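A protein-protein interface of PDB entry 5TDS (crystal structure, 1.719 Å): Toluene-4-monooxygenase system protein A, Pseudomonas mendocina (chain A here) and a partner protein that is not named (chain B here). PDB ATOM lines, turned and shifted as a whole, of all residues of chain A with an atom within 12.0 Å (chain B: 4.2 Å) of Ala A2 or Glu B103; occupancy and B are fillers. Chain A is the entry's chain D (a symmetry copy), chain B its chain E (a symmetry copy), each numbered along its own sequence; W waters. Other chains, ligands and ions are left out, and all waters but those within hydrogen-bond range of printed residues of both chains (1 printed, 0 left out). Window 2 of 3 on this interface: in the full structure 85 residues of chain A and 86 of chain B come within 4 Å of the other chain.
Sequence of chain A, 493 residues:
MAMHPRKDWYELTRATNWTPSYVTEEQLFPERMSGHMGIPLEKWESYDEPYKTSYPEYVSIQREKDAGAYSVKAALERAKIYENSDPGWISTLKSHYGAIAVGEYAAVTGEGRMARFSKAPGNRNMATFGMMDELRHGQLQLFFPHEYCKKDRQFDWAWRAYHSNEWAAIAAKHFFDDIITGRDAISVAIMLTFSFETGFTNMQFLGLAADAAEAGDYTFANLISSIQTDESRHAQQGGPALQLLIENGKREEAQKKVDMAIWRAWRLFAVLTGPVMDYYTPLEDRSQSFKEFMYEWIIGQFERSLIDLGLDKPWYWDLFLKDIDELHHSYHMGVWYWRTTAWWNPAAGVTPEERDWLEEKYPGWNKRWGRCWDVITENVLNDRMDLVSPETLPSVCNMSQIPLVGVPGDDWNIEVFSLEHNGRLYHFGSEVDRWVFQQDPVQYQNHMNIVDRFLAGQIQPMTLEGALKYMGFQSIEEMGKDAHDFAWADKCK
The side-chain carboxylate (OD1) of Asp B99 lies within hydrogen-bond range of the backbone NH (N) of Ala A2 (2.7 Å).
The backbone NH of Ala A2 sits close to the side-chain amide nitrogen of Asn B102 (2.8 Å).
OE1 of Glu B103 sits at hydrogen-bond distance from N of Ala A2, 2.7 Å away.
N of Asp B99 lies close to SD of Met A3 (3.7 Å).
A ring nitrogen (NE2) of His A4 sits at hydrogen-bond distance from the side-chain amide oxygen of Asn B102 (3.4 Å).
The backbone NH (N) of His A4 is in hydrogen-bond range of the side-chain hydroxyl (OH) of Tyr B168 (3.0 Å).
NE1 of Trp A9 is in hydrogen-bond range of O of His A4, 2.9 Å away.
The indole nitrogen (NE1) of Trp A9 lies within hydrogen-bond range of the backbone carbonyl oxygen (O) of Pro A5, at 3.2 Å.
Among the printed residues, merely in contact across the chains: Trp A9 with Tyr B168 and Met A3 with Tyr B168.
Of the printed residues of chain B, Ala A2 touches Asp B99, Asn B102 and Glu B103.
Of the printed residues of chain B, Met A3 touches Asp B99 and Tyr B168.
Printed residues of chain B within 4 Å of His A4: Asn B102 (3.4 Å) and Tyr B168 (3.0 Å).
Of the printed residues of chain B, Trp A9 touches Tyr B168.
Asp B99 touches two residues of chain A.
Asn B102 touches just these residues of chain A: Ala A2 (2.8 Å) and His A4 (3.4 Å).
Glu B103 touches just one residue of chain A: Ala A2 (2.7 Å).
No residue of chain A comes within 4 Å of Glu B105.
Of the printed residues of chain A, Tyr B168 touches Met A3, His A4 and Trp A9.
The nearest printed residue of chain B that does not touch Ala A2 is Tyr B168 (4.2 Å).
Of the 7 printed residues of chain A, 4 touch a printed residue of chain B.
Printed residues of chain A that touch a printed residue of chain B: Ala A2, Met A3, His A4 and Trp A9.
Hydrophobic or aromatic side chains of chain A within 4 Å of the printed part of chain B: Ala A2, Met A3, His A4 and Trp A9.
Water W1 lies within hydrogen-bond range of the side-chain hydroxyl (OH) of Tyr B168 (2.5 Å) and the backbone carbonyl oxygen (O) of Ala A2 (2.8 Å).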
ATOM      1  N   ALA A   2      18.048  -4.285  32.326  1.00  0.00           N
ATOM      2  CA  ALA A   2      18.370  -2.956  31.807  1.00  0.00           C
ATOM      3  C   ALA A   2      17.443  -2.581  30.662  1.00  0.00           C
ATOM      4  O   ALA A   2      16.828  -3.451  30.047  1.00  0.00           O
ATOM      5  CB  ALA A   2      19.807  -2.902  31.341  1.00  0.00           C
ATOM      6  N   MET A   3      17.358  -1.280  30.389  1.00  0.00           N
ATOM      7  CA  MET A   3      16.608  -0.756  29.247  1.00  0.00           C
ATOM      8  C   MET A   3      17.577  -0.256  28.179  1.00  0.00           C
ATOM      9  O   MET A   3      18.643   0.274  28.502  1.00  0.00           O
ATOM     10  CB  MET A   3      15.674   0.384  29.678  1.00  0.00           C
ATOM     11  CG  MET A   3      14.696   0.029  30.782  1.00  0.00           C
ATOM     12  SD  MET A   3      13.592  -1.286  30.266  1.00  0.00           S
ATOM     13  CE  MET A   3      12.647  -0.434  28.998  1.00  0.00           C
ATOM     14  N   HIS A   4      17.211  -0.420  26.912  1.00  0.00           N
ATOM     15  CA  HIS A   4      18.046   0.070  25.822  1.00  0.00           C
ATOM     16  C   HIS A   4      17.580   1.448  25.401  1.00  0.00           C
ATOM     17  O   HIS A   4      16.380   1.682  25.256  1.00  0.00           O
ATOM     18  CB  HIS A   4      18.005  -0.906  24.652  1.00  0.00           C
ATOM     19  CG  HIS A   4      18.273  -2.317  25.065  1.00  0.00           C
ATOM     20  ND1 HIS A   4      19.497  -2.728  25.547  1.00  0.00           N
ATOM     21  CD2 HIS A   4      17.462  -3.398  25.128  1.00  0.00           C
ATOM     22  CE1 HIS A   4      19.435  -4.009  25.864  1.00  0.00           C
ATOM     23  NE2 HIS A   4      18.210  -4.442  25.613  1.00  0.00           N
ATOM     24  N   PRO A   5      18.530   2.375  25.236  1.00  0.00           N
ATOM     25  CA  PRO A   5      18.234   3.759  24.872  1.00  0.00           C
ATOM     26  C   PRO A   5      17.501   3.844  23.540  1.00  0.00           C
ATOM     27  O   PRO A   5      17.655   2.982  22.677  1.00  0.00           O
ATOM     28  CB  PRO A   5      19.619   4.416  24.789  1.00  0.00           C
ATOM     29  CG  PRO A   5      20.583   3.297  24.668  1.00  0.00           C
ATOM     30  CD  PRO A   5      19.972   2.147  25.416  1.00  0.00           C
ATOM     31  N   ARG A   6      16.702   4.888  23.392  1.00  0.00           N
ATOM     32  CA  ARG A   6      15.821   5.026  22.248  1.00  0.00           C
ATOM     33  C   ARG A   6      16.566   4.982  20.911  1.00  0.00           C
ATOM     34  O   ARG A   6      16.050   4.457  19.932  1.00  0.00           O
ATOM     35  CB  ARG A   6      15.029   6.328  22.366  1.00  0.00           C
ATOM     36  CG  ARG A   6      13.892   6.430  21.391  1.00  0.00           C
ATOM     37  CD  ARG A   6      13.182   7.746  21.598  1.00  0.00           C
ATOM     38  NE  ARG A   6      14.102   8.854  21.387  1.00  0.00           N
ATOM     39  CZ  ARG A   6      14.087   9.986  22.077  1.00  0.00           C
ATOM     40  NH1 ARG A   6      13.202  10.169  23.045  1.00  0.00           N
ATOM     41  NH2 ARG A   6      14.960  10.939  21.790  1.00  0.00           N
ATOM     42  N   ASP A   8      18.815   3.166  19.983  1.00  0.00           N
ATOM     43  CA  ASP A   8      19.158   1.794  19.592  1.00  0.00           C
ATOM     44  C   ASP A   8      18.039   1.108  18.805  1.00  0.00           C
ATOM     45  O   ASP A   8      18.300   0.188  18.022  1.00  0.00           O
ATOM     46  CB  ASP A   8      19.492   0.939  20.822  1.00  0.00           C
ATOM     47  CG  ASP A   8      20.862   1.239  21.403  1.00  0.00           C
ATOM     48  OD1 ASP A   8      21.615   2.037  20.802  1.00  0.00           O
ATOM     49  OD2 ASP A   8      21.189   0.653  22.461  1.00  0.00           O
ATOM     50  N   TRP A   9      16.797   1.546  19.008  1.00  0.00           N
ATOM     51  CA  TRP A   9      15.658   0.836  18.420  1.00  0.00           C
ATOM     52  C   TRP A   9      14.676   1.739  17.683  1.00  0.00           C
ATOM     53  O   TRP A   9      13.752   1.247  17.034  1.00  0.00           O
ATOM     54  CB  TRP A   9      14.906   0.047  19.503  1.00  0.00           C
ATOM     55  CG  TRP A   9      14.591   0.829  20.745  1.00  0.00           C
ATOM     56  CD1 TRP A   9      15.332   0.875  21.893  1.00  0.00           C
ATOM     57  CD2 TRP A   9      13.456   1.672  20.967  1.00  0.00           C
ATOM     58  NE1 TRP A   9      14.733   1.701  22.812  1.00  0.00           N
ATOM     59  CE2 TRP A   9      13.574   2.197  22.269  1.00  0.00           C
ATOM     60  CE3 TRP A   9      12.351   2.037  20.188  1.00  0.00           C
ATOM     61  CZ2 TRP A   9      12.635   3.070  22.811  1.00  0.00           C
ATOM     62  CZ3 TRP A   9      11.413   2.902  20.732  1.00  0.00           C
ATOM     63  CH2 TRP A   9      11.565   3.412  22.031  1.00  0.00           C
ATOM     64  N   ASP B  99      12.755  -4.637  31.479  1.00  0.00           N
ATOM     65  CA  ASP B  99      13.945  -4.379  32.289  1.00  0.00           C
ATOM     66  C   ASP B  99      14.371  -5.636  33.040  1.00  0.00           C
ATOM     67  O   ASP B  99      15.538  -6.019  32.999  1.00  0.00           O
ATOM     68  CB  ASP B  99      13.672  -3.223  33.262  1.00  0.00           C
ATOM     69  CG  ASP B  99      14.888  -2.839  34.099  1.00  0.00           C
ATOM     70  OD1 ASP B  99      16.034  -2.995  33.642  1.00  0.00           O
ATOM     71  OD2 ASP B  99      14.683  -2.346  35.228  1.00  0.00           O
ATOM     72  N   GLN B 100      13.422  -6.283  33.709  1.00  0.00           N
ATOM     73  CA  GLN B 100      13.723  -7.450  34.545  1.00  0.00           C
ATOM     74  C   GLN B 100      14.116  -8.688  33.731  1.00  0.00           C
ATOM     75  O   GLN B 100      15.019  -9.432  34.115  1.00  0.00           O
ATOM     76  CB  GLN B 100      12.520  -7.789  35.429  1.00  0.00           C
ATOM     77  CG  GLN B 100      12.074  -6.656  36.313  1.00  0.00           C
ATOM     78  CD  GLN B 100      10.626  -6.796  36.743  1.00  0.00           C
ATOM     79  OE1 GLN B 100      10.020  -5.836  37.233  1.00  0.00           O
ATOM     80  NE2 GLN B 100      10.057  -7.986  36.554  1.00  0.00           N
ATOM     81  N   PHE B 101      13.422  -8.926  32.624  1.00  0.00           N
ATOM     82  CA  PHE B 101      13.747 -10.085  31.805  1.00  0.00           C
ATOM     83  C   PHE B 101      15.119  -9.885  31.176  1.00  0.00           C
ATOM     84  O   PHE B 101      15.890 -10.833  31.039  1.00  0.00           O
ATOM     85  CB  PHE B 101      12.666 -10.330  30.738  1.00  0.00           C
ATOM     86  CG  PHE B 101      11.472 -11.098  31.262  1.00  0.00           C
ATOM     87  CD1 PHE B 101      11.468 -12.478  31.260  1.00  0.00           C
ATOM     88  CD2 PHE B 101      10.369 -10.442  31.771  1.00  0.00           C
ATOM     89  CE1 PHE B 101      10.382 -13.196  31.744  1.00  0.00           C
ATOM     90  CE2 PHE B 101       9.279 -11.157  32.255  1.00  0.00           C
ATOM     91  CZ  PHE B 101       9.291 -12.532  32.246  1.00  0.00           C
ATOM     92  N   ASN B 102      15.429  -8.646  30.808  1.00  0.00           N
ATOM     93  CA  ASN B 102      16.741  -8.347  30.253  1.00  0.00           C
ATOM     94  C   ASN B 102      17.828  -8.627  31.289  1.00  0.00           C
ATOM     95  O   ASN B 102      18.884  -9.192  30.970  1.00  0.00           O
ATOM     96  CB  ASN B 102      16.811  -6.893  29.784  1.00  0.00           C
ATOM     97  CG  ASN B 102      18.217  -6.472  29.408  1.00  0.00           C
ATOM     98  OD1 ASN B 102      18.603  -6.525  28.236  1.00  0.00           O
ATOM     99  ND2 ASN B 102      18.997  -6.054  30.403  1.00  0.00           N
ATOM    100  N   GLU B 103      17.562  -8.241  32.530  1.00  0.00           N
ATOM    101  CA  GLU B 103      18.543  -8.426  33.606  1.00  0.00           C
ATOM    102  C   GLU B 103      18.912  -9.889  33.812  1.00  0.00           C
ATOM    103  O   GLU B 103      20.064 -10.206  34.113  1.00  0.00           O
ATOM    104  CB  GLU B 103      18.020  -7.853  34.924  1.00  0.00           C
ATOM    105  CG  GLU B 103      18.117  -6.342  35.029  1.00  0.00           C
ATOM    106  CD  GLU B 103      19.554  -5.847  35.011  1.00  0.00           C
ATOM    107  OE1 GLU B 103      19.844  -4.901  34.248  1.00  0.00           O
ATOM    108  OE2 GLU B 103      20.391  -6.403  35.762  1.00  0.00           O
ATOM    109  N   ARG B 104      17.942 -10.784  33.666  1.00  0.00           N
ATOM    110  CA  ARG B 104      18.216 -12.196  33.911  1.00  0.00           C
ATOM    111  C   ARG B 104      18.520 -12.957  32.612  1.00  0.00           C
ATOM    112  O   ARG B 104      18.587 -14.196  32.601  1.00  0.00           O
ATOM    113  CB  ARG B 104      17.050 -12.848  34.659  1.00  0.00           C
ATOM    114  CG  ARG B 104      15.777 -12.957  33.882  1.00  0.00           C
ATOM    115  CD  ARG B 104      14.748 -13.784  34.645  1.00  0.00           C
ATOM    116  NE  ARG B 104      14.175 -13.049  35.766  1.00  0.00           N
ATOM    117  CZ  ARG B 104      13.051 -12.343  35.693  1.00  0.00           C
ATOM    118  NH1 ARG B 104      12.600 -11.698  36.759  1.00  0.00           N
ATOM    119  NH2 ARG B 104      12.374 -12.284  34.555  1.00  0.00           N
ATOM    120  N   GLU B 105      18.733 -12.208  31.532  1.00  0.00           N
ATOM    121  CA  GLU B 105      19.155 -12.789  30.258  1.00  0.00           C
ATOM    122  C   GLU B 105      18.166 -13.865  29.821  1.00  0.00           C
ATOM    123  O   GLU B 105      18.550 -14.959  29.396  1.00  0.00           O
ATOM    124  CB  GLU B 105      20.570 -13.371  30.368  1.00  0.00           C
ATOM    125  CG  GLU B 105      21.626 -12.346  30.795  1.00  0.00           C
ATOM    126  CD  GLU B 105      21.894 -11.292  29.731  1.00  0.00           C
ATOM    127  OE1 GLU B 105      21.397 -11.449  28.595  1.00  0.00           O
ATOM    128  OE2 GLU B 105      22.607 -10.308  30.026  1.00  0.00           O
ATOM    129  N   TYR B 168      11.071  -2.444  19.802  1.00  0.00           N
ATOM    130  CA  TYR B 168      11.956  -2.570  20.953  1.00  0.00           C
ATOM    131  C   TYR B 168      12.454  -4.001  21.090  1.00  0.00           C
ATOM    132  O   TYR B 168      13.647  -4.240  21.270  1.00  0.00           O
ATOM    133  CB  TYR B 168      11.246  -2.144  22.245  1.00  0.00           C
ATOM    134  CG  TYR B 168      12.174  -2.127  23.434  1.00  0.00           C
ATOM    135  CD1 TYR B 168      12.386  -3.281  24.198  1.00  0.00           C
ATOM    136  CD2 TYR B 168      12.846  -0.966  23.793  1.00  0.00           C
ATOM    137  CE1 TYR B 168      13.245  -3.277  25.284  1.00  0.00           C
ATOM    138  CE2 TYR B 168      13.714  -0.953  24.894  1.00  0.00           C
ATOM    139  CZ  TYR B 168      13.903  -2.109  25.626  1.00  0.00           C
ATOM    140  OH  TYR B 168      14.748  -2.094  26.704  1.00  0.00           O
HETATM  141  O   HOH W   1      14.972  -4.189  28.065  1.00  0.00           O
